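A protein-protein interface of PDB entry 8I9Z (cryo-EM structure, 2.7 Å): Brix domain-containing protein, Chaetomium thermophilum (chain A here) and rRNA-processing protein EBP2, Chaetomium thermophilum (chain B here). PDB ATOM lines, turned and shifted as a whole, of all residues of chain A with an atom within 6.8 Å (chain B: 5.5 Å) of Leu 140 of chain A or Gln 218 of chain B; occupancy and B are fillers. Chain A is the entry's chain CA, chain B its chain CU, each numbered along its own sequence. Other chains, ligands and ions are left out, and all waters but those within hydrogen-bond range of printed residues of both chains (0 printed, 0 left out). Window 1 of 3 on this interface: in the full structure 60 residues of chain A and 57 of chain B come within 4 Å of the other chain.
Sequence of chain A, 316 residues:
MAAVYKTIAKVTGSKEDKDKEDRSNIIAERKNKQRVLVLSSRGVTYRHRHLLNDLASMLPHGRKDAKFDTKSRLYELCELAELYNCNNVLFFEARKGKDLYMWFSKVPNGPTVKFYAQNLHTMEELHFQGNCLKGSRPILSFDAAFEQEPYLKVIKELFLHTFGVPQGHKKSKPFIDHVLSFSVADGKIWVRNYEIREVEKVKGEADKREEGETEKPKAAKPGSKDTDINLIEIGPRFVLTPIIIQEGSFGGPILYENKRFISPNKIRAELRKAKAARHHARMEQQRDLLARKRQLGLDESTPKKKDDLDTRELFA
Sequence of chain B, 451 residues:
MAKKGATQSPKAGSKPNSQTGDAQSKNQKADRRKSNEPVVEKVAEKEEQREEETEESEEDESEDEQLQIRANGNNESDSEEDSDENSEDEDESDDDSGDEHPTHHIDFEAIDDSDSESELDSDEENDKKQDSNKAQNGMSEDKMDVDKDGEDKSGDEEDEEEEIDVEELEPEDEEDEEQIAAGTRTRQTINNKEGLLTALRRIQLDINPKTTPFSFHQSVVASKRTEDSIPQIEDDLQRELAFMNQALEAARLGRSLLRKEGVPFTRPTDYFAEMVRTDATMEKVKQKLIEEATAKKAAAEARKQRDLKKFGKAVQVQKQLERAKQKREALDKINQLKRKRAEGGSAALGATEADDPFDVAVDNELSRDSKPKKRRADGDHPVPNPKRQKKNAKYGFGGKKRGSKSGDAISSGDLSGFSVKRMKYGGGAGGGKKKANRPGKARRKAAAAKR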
ATOM      1  N   ARG A 137     -20.442 -11.333  15.930  1.00  0.00           N
ATOM      2  CA  ARG A 137     -20.274  -9.890  15.899  1.00  0.00           C
ATOM      3  C   ARG A 137     -19.436  -9.493  14.693  1.00  0.00           C
ATOM      4  O   ARG A 137     -18.273  -9.898  14.601  1.00  0.00           O
ATOM      5  CB  ARG A 137     -19.612  -9.405  17.179  1.00  0.00           C
ATOM      6  CG  ARG A 137     -20.320  -9.837  18.440  1.00  0.00           C
ATOM      7  CD  ARG A 137     -19.993  -8.903  19.585  1.00  0.00           C
ATOM      8  NE  ARG A 137     -20.167  -7.507  19.208  1.00  0.00           N
ATOM      9  CZ  ARG A 137     -19.358  -6.526  19.580  1.00  0.00           C
ATOM     10  NH1 ARG A 137     -18.308  -6.753  20.348  1.00  0.00           N
ATOM     11  NH2 ARG A 137     -19.605  -5.289  19.165  1.00  0.00           N
ATOM     12  N   PRO A 138     -19.969  -8.712  13.766  1.00  0.00           N
ATOM     13  CA  PRO A 138     -19.226  -8.388  12.551  1.00  0.00           C
ATOM     14  C   PRO A 138     -18.279  -7.221  12.774  1.00  0.00           C
ATOM     15  O   PRO A 138     -18.373  -6.475  13.749  1.00  0.00           O
ATOM     16  CB  PRO A 138     -20.333  -8.007  11.571  1.00  0.00           C
ATOM     17  CG  PRO A 138     -21.380  -7.408  12.434  1.00  0.00           C
ATOM     18  CD  PRO A 138     -21.292  -8.071  13.784  1.00  0.00           C
ATOM     19  N   ILE A 139     -17.355  -7.073  11.839  1.00  0.00           N
ATOM     20  CA  ILE A 139     -16.555  -5.866  11.717  1.00  0.00           C
ATOM     21  C   ILE A 139     -17.231  -4.996  10.671  1.00  0.00           C
ATOM     22  O   ILE A 139     -17.457  -5.437   9.538  1.00  0.00           O
ATOM     23  CB  ILE A 139     -15.101  -6.183  11.336  1.00  0.00           C
ATOM     24  CG1 ILE A 139     -14.334  -6.697  12.553  1.00  0.00           C
ATOM     25  CG2 ILE A 139     -14.412  -4.953  10.771  1.00  0.00           C
ATOM     26  CD1 ILE A 139     -12.887  -7.003  12.276  1.00  0.00           C
ATOM     27  N   LEU A 140     -17.578  -3.774  11.045  1.00  0.00           N
ATOM     28  CA  LEU A 140     -18.270  -2.866  10.145  1.00  0.00           C
ATOM     29  C   LEU A 140     -17.246  -2.065   9.355  1.00  0.00           C
ATOM     30  O   LEU A 140     -16.491  -1.275   9.928  1.00  0.00           O
ATOM     31  CB  LEU A 140     -19.202  -1.944  10.926  1.00  0.00           C
ATOM     32  CG  LEU A 140     -20.376  -2.616  11.641  1.00  0.00           C
ATOM     33  CD1 LEU A 140     -21.378  -1.578  12.100  1.00  0.00           C
ATOM     34  CD2 LEU A 140     -21.044  -3.644  10.752  1.00  0.00           C
ATOM     35  N   SER A 141     -17.214  -2.275   8.046  1.00  0.00           N
ATOM     36  CA  SER A 141     -16.358  -1.513   7.154  1.00  0.00           C
ATOM     37  C   SER A 141     -17.156  -0.363   6.563  1.00  0.00           C
ATOM     38  O   SER A 141     -18.135  -0.586   5.843  1.00  0.00           O
ATOM     39  CB  SER A 141     -15.804  -2.393   6.036  1.00  0.00           C
ATOM     40  OG  SER A 141     -15.292  -1.604   4.978  1.00  0.00           O
ATOM     41  N   PHE A 142     -16.742   0.856   6.866  1.00  0.00           N
ATOM     42  CA  PHE A 142     -17.362   2.049   6.321  1.00  0.00           C
ATOM     43  C   PHE A 142     -16.390   2.710   5.352  1.00  0.00           C
ATOM     44  O   PHE A 142     -15.255   2.265   5.172  1.00  0.00           O
ATOM     45  CB  PHE A 142     -17.772   3.007   7.441  1.00  0.00           C
ATOM     46  CG  PHE A 142     -19.009   2.586   8.171  1.00  0.00           C
ATOM     47  CD1 PHE A 142     -20.262   2.820   7.639  1.00  0.00           C
ATOM     48  CD2 PHE A 142     -18.916   1.948   9.391  1.00  0.00           C
ATOM     49  CE1 PHE A 142     -21.399   2.424   8.314  1.00  0.00           C
ATOM     50  CE2 PHE A 142     -20.044   1.551  10.069  1.00  0.00           C
ATOM     51  CZ  PHE A 142     -21.286   1.788   9.531  1.00  0.00           C
ATOM     52  N   LYS A 156     -24.556   6.499   8.786  1.00  0.00           N
ATOM     53  CA  LYS A 156     -23.559   5.610   9.374  1.00  0.00           C
ATOM     54  C   LYS A 156     -23.927   5.220  10.800  1.00  0.00           C
ATOM     55  O   LYS A 156     -23.782   4.054  11.188  1.00  0.00           O
ATOM     56  CB  LYS A 156     -22.184   6.274   9.337  1.00  0.00           C
ATOM     57  CG  LYS A 156     -21.151   5.594  10.206  1.00  0.00           C
ATOM     58  CD  LYS A 156     -19.812   6.288  10.154  1.00  0.00           C
ATOM     59  CE  LYS A 156     -18.829   5.596  11.073  1.00  0.00           C
ATOM     60  NZ  LYS A 156     -19.236   5.726  12.496  1.00  0.00           N
ATOM     61  N   PHE A 159     -26.617   2.775  10.683  1.00  0.00           N
ATOM     62  CA  PHE A 159     -26.072   1.480  10.292  1.00  0.00           C
ATOM     63  C   PHE A 159     -25.315   0.828  11.442  1.00  0.00           C
ATOM     64  O   PHE A 159     -25.249  -0.401  11.530  1.00  0.00           O
ATOM     65  CB  PHE A 159     -25.158   1.646   9.081  1.00  0.00           C
ATOM     66  CG  PHE A 159     -25.886   1.718   7.775  1.00  0.00           C
ATOM     67  CD1 PHE A 159     -27.236   1.450   7.701  1.00  0.00           C
ATOM     68  CD2 PHE A 159     -25.213   2.059   6.619  1.00  0.00           C
ATOM     69  CE1 PHE A 159     -27.902   1.517   6.500  1.00  0.00           C
ATOM     70  CE2 PHE A 159     -25.877   2.129   5.415  1.00  0.00           C
ATOM     71  CZ  PHE A 159     -27.221   1.861   5.357  1.00  0.00           C
ATOM     72  N   LEU A 160     -24.719   1.635  12.322  1.00  0.00           N
ATOM     73  CA  LEU A 160     -23.989   1.080  13.456  1.00  0.00           C
ATOM     74  C   LEU A 160     -24.943   0.593  14.539  1.00  0.00           C
ATOM     75  O   LEU A 160     -24.604  -0.305  15.314  1.00  0.00           O
ATOM     76  CB  LEU A 160     -23.019   2.120  14.012  1.00  0.00           C
ATOM     77  CG  LEU A 160     -21.894   1.629  14.920  1.00  0.00           C
ATOM     78  CD1 LEU A 160     -20.602   2.315  14.536  1.00  0.00           C
ATOM     79  CD2 LEU A 160     -22.209   1.881  16.381  1.00  0.00           C
ATOM     80  N   HIS A 161     -26.132   1.190  14.620  1.00  0.00           N
ATOM     81  CA  HIS A 161     -27.128   0.721  15.576  1.00  0.00           C
ATOM     82  C   HIS A 161     -27.827  -0.541  15.084  1.00  0.00           C
ATOM     83  O   HIS A 161     -28.087  -1.459  15.868  1.00  0.00           O
ATOM     84  CB  HIS A 161     -28.149   1.824  15.851  1.00  0.00           C
ATOM     85  CG  HIS A 161     -27.610   2.971  16.651  1.00  0.00           C
ATOM     86  ND1 HIS A 161     -28.402   3.729  17.486  1.00  0.00           N
ATOM     87  CD2 HIS A 161     -26.356   3.466  16.777  1.00  0.00           C
ATOM     88  CE1 HIS A 161     -27.666   4.659  18.067  1.00  0.00           C
ATOM     89  NE2 HIS A 161     -26.421   4.521  17.652  1.00  0.00           N
ATOM     90  N   PHE A 163     -26.843  -2.870  12.641  1.00  0.00           N
ATOM     91  CA  PHE A 163     -25.958  -4.013  12.458  1.00  0.00           C
ATOM     92  C   PHE A 163     -24.874  -4.086  13.527  1.00  0.00           C
ATOM     93  O   PHE A 163     -23.781  -4.591  13.261  1.00  0.00           O
ATOM     94  CB  PHE A 163     -25.324  -3.973  11.071  1.00  0.00           C
ATOM     95  CG  PHE A 163     -26.315  -3.903   9.954  1.00  0.00           C
ATOM     96  CD1 PHE A 163     -27.189  -4.949   9.719  1.00  0.00           C
ATOM     97  CD2 PHE A 163     -26.358  -2.802   9.121  1.00  0.00           C
ATOM     98  CE1 PHE A 163     -28.095  -4.890   8.683  1.00  0.00           C
ATOM     99  CE2 PHE A 163     -27.262  -2.738   8.082  1.00  0.00           C
ATOM    100  CZ  PHE A 163     -28.130  -3.783   7.863  1.00  0.00           C
ATOM    101  N   GLY A 164     -25.158  -3.594  14.732  1.00  0.00           N
ATOM    102  CA  GLY A 164     -24.127  -3.512  15.750  1.00  0.00           C
ATOM    103  C   GLY A 164     -23.741  -4.853  16.341  1.00  0.00           C
ATOM    104  O   GLY A 164     -22.551  -5.174  16.429  1.00  0.00           O
ATOM    105  N   VAL A 165     -24.732  -5.658  16.723  1.00  0.00           N
ATOM    106  CA  VAL A 165     -24.570  -6.872  17.529  1.00  0.00           C
ATOM    107  C   VAL A 165     -23.799  -6.539  18.802  1.00  0.00           C
ATOM    108  O   VAL A 165     -22.571  -6.711  18.840  1.00  0.00           O
ATOM    109  CB  VAL A 165     -23.911  -8.015  16.741  1.00  0.00           C
ATOM    110  CG1 VAL A 165     -23.999  -9.307  17.526  1.00  0.00           C
ATOM    111  CG2 VAL A 165     -24.587  -8.176  15.399  1.00  0.00           C
ATOM    112  N   GLN A 167     -22.001  -6.101  22.603  1.00  0.00           N
ATOM    113  CA  GLN A 167     -20.781  -6.840  22.919  1.00  0.00           C
ATOM    114  C   GLN A 167     -21.059  -8.100  23.729  1.00  0.00           C
ATOM    115  O   GLN A 167     -20.558  -9.181  23.401  1.00  0.00           O
ATOM    116  CB  GLN A 167     -19.802  -5.930  23.656  1.00  0.00           C
ATOM    117  CG  GLN A 167     -18.399  -6.478  23.754  1.00  0.00           C
ATOM    118  CD  GLN A 167     -17.507  -5.643  24.644  1.00  0.00           C
ATOM    119  OE1 GLN A 167     -17.793  -4.479  24.912  1.00  0.00           O
ATOM    120  NE2 GLN A 167     -16.415  -6.234  25.107  1.00  0.00           N
ATOM    121  N   ILE A 176     -14.966 -14.179  15.561  1.00  0.00           N
ATOM    122  CA  ILE A 176     -15.157 -13.214  14.484  1.00  0.00           C
ATOM    123  C   ILE A 176     -14.730 -13.845  13.168  1.00  0.00           C
ATOM    124  O   ILE A 176     -13.573 -14.252  13.014  1.00  0.00           O
ATOM    125  CB  ILE A 176     -14.380 -11.922  14.754  1.00  0.00           C
ATOM    126  CG1 ILE A 176     -14.907 -11.285  16.042  1.00  0.00           C
ATOM    127  CG2 ILE A 176     -14.469 -10.994  13.550  1.00  0.00           C
ATOM    128  CD1 ILE A 176     -14.716  -9.810  16.145  1.00  0.00           C
ATOM    129  N   HIS A 178     -16.615 -12.651   9.913  1.00  0.00           N
ATOM    130  CA  HIS A 178     -17.170 -11.963   8.759  1.00  0.00           C
ATOM    131  C   HIS A 178     -17.170 -10.458   8.974  1.00  0.00           C
ATOM    132  O   HIS A 178     -17.199  -9.971  10.106  1.00  0.00           O
ATOM    133  CB  HIS A 178     -18.578 -12.472   8.417  1.00  0.00           C
ATOM    134  CG  HIS A 178     -19.682 -11.845   9.208  1.00  0.00           C
ATOM    135  ND1 HIS A 178     -20.010 -12.252  10.482  1.00  0.00           N
ATOM    136  CD2 HIS A 178     -20.562 -10.869   8.887  1.00  0.00           C
ATOM    137  CE1 HIS A 178     -21.034 -11.542  10.919  1.00  0.00           C
ATOM    138  NE2 HIS A 178     -21.387 -10.696   9.969  1.00  0.00           N
ATOM    139  N   VAL A 179     -17.130  -9.731   7.860  1.00  0.00           N
ATOM    140  CA  VAL A 179     -17.066  -8.276   7.843  1.00  0.00           C
ATOM    141  C   VAL A 179     -18.158  -7.759   6.919  1.00  0.00           C
ATOM    142  O   VAL A 179     -18.285  -8.220   5.780  1.00  0.00           O
ATOM    143  CB  VAL A 179     -15.675  -7.775   7.398  1.00  0.00           C
ATOM    144  CG1 VAL A 179     -15.086  -8.691   6.342  1.00  0.00           C
ATOM    145  CG2 VAL A 179     -15.737  -6.349   6.880  1.00  0.00           C
ATOM    146  N   LEU A 180     -18.953  -6.816   7.414  1.00  0.00           N
ATOM    147  CA  LEU A 180     -20.022  -6.185   6.653  1.00  0.00           C
ATOM    148  C   LEU A 180     -19.520  -4.833   6.167  1.00  0.00           C
ATOM    149  O   LEU A 180     -19.080  -4.009   6.974  1.00  0.00           O
ATOM    150  CB  LEU A 180     -21.271  -6.032   7.518  1.00  0.00           C
ATOM    151  CG  LEU A 180     -22.627  -5.868   6.842  1.00  0.00           C
ATOM    152  CD1 LEU A 180     -23.007  -7.130   6.094  1.00  0.00           C
ATOM    153  CD2 LEU A 180     -23.675  -5.527   7.882  1.00  0.00           C
ATOM    154  N   SER A 181     -19.573  -4.610   4.859  1.00  0.00           N
ATOM    155  CA  SER A 181     -18.954  -3.447   4.240  1.00  0.00           C
ATOM    156  C   SER A 181     -20.002  -2.531   3.623  1.00  0.00           C
ATOM    157  O   SER A 181     -20.990  -2.996   3.049  1.00  0.00           O
ATOM    158  CB  SER A 181     -17.950  -3.871   3.168  1.00  0.00           C
ATOM    159  OG  SER A 181     -18.611  -4.275   1.985  1.00  0.00           O
ATOM    160  N   PHE A 182     -19.774  -1.226   3.745  1.00  0.00           N
ATOM    161  CA  PHE A 182     -20.604  -0.201   3.127  1.00  0.00           C
ATOM    162  C   PHE A 182     -19.707   0.742   2.341  1.00  0.00           C
ATOM    163  O   PHE A 182     -18.687   1.205   2.858  1.00  0.00           O
ATOM    164  CB  PHE A 182     -21.410   0.581   4.169  1.00  0.00           C
ATOM    165  CG  PHE A 182     -22.069  -0.280   5.204  1.00  0.00           C
ATOM    166  CD1 PHE A 182     -23.310  -0.835   4.968  1.00  0.00           C
ATOM    167  CD2 PHE A 182     -21.454  -0.525   6.417  1.00  0.00           C
ATOM    168  CE1 PHE A 182     -23.921  -1.625   5.918  1.00  0.00           C
ATOM    169  CE2 PHE A 182     -22.062  -1.313   7.369  1.00  0.00           C
ATOM    170  CZ  PHE A 182     -23.295  -1.861   7.118  1.00  0.00           C
ATOM    171  N   PHE B 214     -12.260  -1.102  21.138  1.00  0.00           N
ATOM    172  CA  PHE B 214     -12.697  -1.459  19.793  1.00  0.00           C
ATOM    173  C   PHE B 214     -13.721  -2.582  19.815  1.00  0.00           C
ATOM    174  O   PHE B 214     -14.522  -2.710  18.884  1.00  0.00           O
ATOM    175  CB  PHE B 214     -11.494  -1.855  18.941  1.00  0.00           C
ATOM    176  CG  PHE B 214     -11.839  -2.194  17.522  1.00  0.00           C
ATOM    177  CD1 PHE B 214     -12.149  -1.199  16.616  1.00  0.00           C
ATOM    178  CD2 PHE B 214     -11.842  -3.509  17.092  1.00  0.00           C
ATOM    179  CE1 PHE B 214     -12.460  -1.506  15.313  1.00  0.00           C
ATOM    180  CE2 PHE B 214     -12.155  -3.824  15.789  1.00  0.00           C
ATOM    181  CZ  PHE B 214     -12.462  -2.821  14.898  1.00  0.00           C
ATOM    182  N   SER B 215     -13.717  -3.400  20.870  1.00  0.00           N
ATOM    183  CA  SER B 215     -14.697  -4.475  20.981  1.00  0.00           C
ATOM    184  C   SER B 215     -16.102  -3.934  21.202  1.00  0.00           C
ATOM    185  O   SER B 215     -17.086  -4.644  20.962  1.00  0.00           O
ATOM    186  CB  SER B 215     -14.306  -5.420  22.114  1.00  0.00           C
ATOM    187  OG  SER B 215     -14.051  -4.702  23.307  1.00  0.00           O
ATOM    188  N   PHE B 216     -16.216  -2.689  21.658  1.00  0.00           N
ATOM    189  CA  PHE B 216     -17.515  -2.056  21.847  1.00  0.00           C
ATOM    190  C   PHE B 216     -18.198  -1.762  20.517  1.00  0.00           C
ATOM    191  O   PHE B 216     -19.412  -1.940  20.380  1.00  0.00           O
ATOM    192  CB  PHE B 216     -17.339  -0.771  22.655  1.00  0.00           C
ATOM    193  CG  PHE B 216     -18.621  -0.063  22.962  1.00  0.00           C
ATOM    194  CD1 PHE B 216     -19.434  -0.485  23.994  1.00  0.00           C
ATOM    195  CD2 PHE B 216     -19.007   1.041  22.222  1.00  0.00           C
ATOM    196  CE1 PHE B 216     -20.610   0.173  24.271  1.00  0.00           C
ATOM    197  CE2 PHE B 216     -20.183   1.696  22.498  1.00  0.00           C
ATOM    198  CZ  PHE B 216     -20.982   1.263  23.523  1.00  0.00           C
ATOM    199  N   HIS B 217     -17.432  -1.313  19.528  1.00  0.00           N
ATOM    200  CA  HIS B 217     -17.992  -0.702  18.331  1.00  0.00           C
ATOM    201  C   HIS B 217     -17.663  -1.459  17.048  1.00  0.00           C
ATOM    202  O   HIS B 217     -18.543  -1.598  16.191  1.00  0.00           O
ATOM    203  CB  HIS B 217     -17.582   0.786  18.333  1.00  0.00           C
ATOM    204  CG  HIS B 217     -16.198   1.089  17.834  1.00  0.00           C
ATOM    205  ND1 HIS B 217     -15.788   0.698  16.577  1.00  0.00           N
ATOM    206  CD2 HIS B 217     -15.097   1.588  18.440  1.00  0.00           C
ATOM    207  CE1 HIS B 217     -14.526   1.041  16.398  1.00  0.00           C
ATOM    208  NE2 HIS B 217     -14.082   1.580  17.516  1.00  0.00           N
ATOM    209  N   GLN B 218     -16.436  -1.974  16.918  1.00  0.00           N
ATOM    210  CA  GLN B 218     -16.012  -2.859  15.823  1.00  0.00           C
ATOM    211  C   GLN B 218     -16.304  -2.279  14.441  1.00  0.00           C
ATOM    212  O   GLN B 218     -16.668  -2.998  13.509  1.00  0.00           O
ATOM    213  CB  GLN B 218     -16.635  -4.246  15.970  1.00  0.00           C
ATOM    214  CG  GLN B 218     -16.031  -5.057  17.097  1.00  0.00           C
ATOM    215  CD  GLN B 218     -16.166  -6.544  16.887  1.00  0.00           C
ATOM    216  OE1 GLN B 218     -16.370  -7.007  15.770  1.00  0.00           O
ATOM    217  NE2 GLN B 218     -16.057  -7.302  17.966  1.00  0.00           N
ATOM    218  N   SER B 219     -16.141  -0.970  14.304  1.00  0.00           N
ATOM    219  CA  SER B 219     -16.325  -0.274  13.043  1.00  0.00           C
ATOM    220  C   SER B 219     -15.035   0.449  12.696  1.00  0.00           C
ATOM    221  O   SER B 219     -14.434   1.098  13.556  1.00  0.00           O
ATOM    222  CB  SER B 219     -17.485   0.719  13.114  1.00  0.00           C
ATOM    223  OG  SER B 219     -17.272   1.679  14.129  1.00  0.00           O
ATOM    224  N   VAL B 220     -14.613   0.329  11.442  1.00  0.00           N
ATOM    225  CA  VAL B 220     -13.401   0.963  10.944  1.00  0.00           C
ATOM    226  C   VAL B 220     -13.780   1.839   9.758  1.00  0.00           C
ATOM    227  O   VAL B 220     -14.501   1.391   8.861  1.00  0.00           O
ATOM    228  CB  VAL B 220     -12.345  -0.080  10.528  1.00  0.00           C
ATOM    229  CG1 VAL B 220     -11.075   0.601  10.040  1.00  0.00           C
ATOM    230  CG2 VAL B 220     -12.037  -1.018  11.677  1.00  0.00           C
ATOM    231  N   VAL B 221     -13.299   3.080   9.752  1.00  0.00           N
ATOM    232  CA  VAL B 221     -13.512   4.004   8.642  1.00  0.00           C
ATOM    233  C   VAL B 221     -12.251   4.044   7.789  1.00  0.00           C
ATOM    234  O   VAL B 221     -11.152   4.281   8.306  1.00  0.00           O
ATOM    235  CB  VAL B 221     -13.878   5.408   9.148  1.00  0.00           C
ATOM    236  CG1 VAL B 221     -14.114   6.335   7.980  1.00  0.00           C
ATOM    237  CG2 VAL B 221     -15.107   5.344  10.032  1.00  0.00           C
ATOM    238  N   ALA B 250     -10.174  -3.143   6.609  1.00  0.00           N
ATOM    239  CA  ALA B 250     -10.978  -3.140   7.825  1.00  0.00           C
ATOM    240  C   ALA B 250     -10.824  -4.445   8.588  1.00  0.00           C
ATOM    241  O   ALA B 250     -10.834  -4.458   9.824  1.00  0.00           O
ATOM    242  CB  ALA B 250     -12.443  -2.888   7.488  1.00  0.00           C
ATOM    243  N   LEU B 258      -8.204  -6.107  17.773  1.00  0.00           N
ATOM    244  CA  LEU B 258      -8.882  -7.063  18.644  1.00  0.00           C
ATOM    245  C   LEU B 258      -7.891  -7.977  19.350  1.00  0.00           C
ATOM    246  O   LEU B 258      -8.076  -8.308  20.525  1.00  0.00           O
ATOM    247  CB  LEU B 258      -9.888  -7.886  17.844  1.00  0.00           C
ATOM    248  CG  LEU B 258     -11.216  -7.215  17.504  1.00  0.00           C
ATOM    249  CD1 LEU B 258     -11.724  -7.722  16.174  1.00  0.00           C
ATOM    250  CD2 LEU B 258     -12.234  -7.466  18.590  1.00  0.00           C
ATOM    251  N   VAL B 263      -9.535 -10.155  22.806  1.00  0.00           N
ATOM    252  CA  VAL B 263     -10.786 -10.738  22.312  1.00  0.00           C
ATOM    253  C   VAL B 263     -10.459 -11.892  21.370  1.00  0.00           C
ATOM    254  O   VAL B 263      -9.625 -11.726  20.463  1.00  0.00           O
ATOM    255  CB  VAL B 263     -11.626  -9.674  21.610  1.00  0.00           C
ATOM    256  CG1 VAL B 263     -12.883 -10.289  21.026  1.00  0.00           C
ATOM    257  CG2 VAL B 263     -11.980  -8.568  22.579  1.00  0.00           C
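A ring nitrogen (ND1) of His 217 of chain B is in hydrogen-bond range of the backbone NH of Ser 219 of chain B, 2.8 Å away.
The backbone carbonyl oxygen (O) of Leu 258 of chain B lies within hydrogen-bond range of the backbone NH (N) of Val 263 of chain B (3.3 Å).
The backbone NH of Ile 139 of chain A lies within hydrogen-bond range of the backbone carbonyl oxygen of His 178 of chain A (3.4 Å).
The backbone carbonyl oxygen (O) of Ile 139 of chain A sits at hydrogen-bond distance from the backbone NH (N) of Leu 180 of chain A, at 2.9 Å.
The backbone carbonyl oxygen (O) of Leu 180 of chain A sits at hydrogen-bond distance from the backbone NH (N) of Ser 141 of chain A (2.8 Å).
The backbone NH (N) of Phe 182 of chain A sits at hydrogen-bond distance from the backbone carbonyl oxygen (O) of Ser 141 of chain A (2.7 Å).
Of chain B, only Gln 218 (2.7 Å), Ser 219 (3.3 Å) and Val 220 (2.9 Å) come within 4 Å of Leu 140 of chain A.
Gln 218 of chain B touches just these residues of chain A: Arg 137, Pro 138, Ile 139, Leu 140 and Ile 176.
Of the printed residues of chain A, Val 221 of chain B touches Lys 156.
Printed residues of chain A within 4 Å of Phe 216 of chain B: Arg 137 and Gln 167.
Of the printed residues of chain A, Ser 215 of chain B touches Arg 137 (2.5 Å) and Gln 167 (3.3 Å).
Of the printed residues of chain B, Leu 160 of chain A touches Ser 219.
Of the printed residues of chain A, Val 220 of chain B touches Leu 140 (2.9 Å), Ser 141 (3.8 Å) and Phe 142 (3.0 Å).
Phe 182 of chain A touches none of the printed residues of chain B.
The nearest printed residue of chain B that does not touch Leu 140 of chain A is His 217 of chain B (5.0 Å).
The nearest printed residue of chain B that does not touch Arg 137 of chain A is His 217 of chain B (4.5 Å).
The backbone carbonyl oxygen (O) of Ser 215 of chain B sits at hydrogen-bond distance from the guanidinium group (NH1) of Arg 137 of chain A, at 2.5 Å.
The side-chain hydroxyl (OG) of Ser 215 of chain B lies within hydrogen-bond range of the side-chain amide nitrogen (NE2) of Gln 167 of chain A (3.3 Å).
The side-chain amide nitrogen (NE2) of Gln 218 of chain B sits close to the guanidinium group (NH1) of Arg 137 of chain A, 3.3 Å away.
The side-chain amide oxygen (OE1) of Gln 218 of chain B sits close to the backbone carbonyl oxygen (O) of Pro 138 of chain A, at 2.9 Å.
The backbone carbonyl oxygen of Gln 218 of chain B sits at hydrogen-bond distance from the backbone NH of Leu 140 of chain A.
The backbone carbonyl oxygen (O) of Leu 140 of chain A sits at hydrogen-bond distance from the backbone NH (N) of Val 220 of chain B, at 2.9 Å.
The backbone NH of Phe 142 of chain A sits at hydrogen-bond distance from the backbone carbonyl oxygen of Val 220 of chain B.
Of the 11 printed residues of chain B, 8 touch a printed residue of chain A.
Of the 20 printed residues of chain A, 10 touch a printed residue of chain B.
Among the printed residues, 18 pairs touch across the chains.
Among the printed residues, no Asp or Glu carboxylate lies within 4 Å of a Lys or Arg side-chain nitrogen of the other chain.
Arg 137 of chain A touches Phe 216 of chain B.
Gln 218 of chain B touches Ile 139 of chain A (O to CA, 3.4 Å).
O of Ala 250 of chain B touches CG2 of Ile 139 of chain A, at 3.7 Å.
Ser 219 of chain B touches Leu 140 of chain A (CA to O, 3.3 Å).
CA of Ser 141 of chain A touches O of Val 220 of chain B, 3.8 Å away.
CB of Ala 250 of chain B touches CB of Ser 141 of chain A (3.7 Å).
Lys 156 of chain A touches Val 221 of chain B.
Leu 160 of chain A touches Ser 219 of chain B (CD1 to OG, 3.4 Å).
OE1 of Gln 167 of chain A touches CA of Phe 216 of chain B, at 3.9 Å.
Ile 176 of chain A touches Leu 258 of chain B (CD1 to CD1, 3.6 Å).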
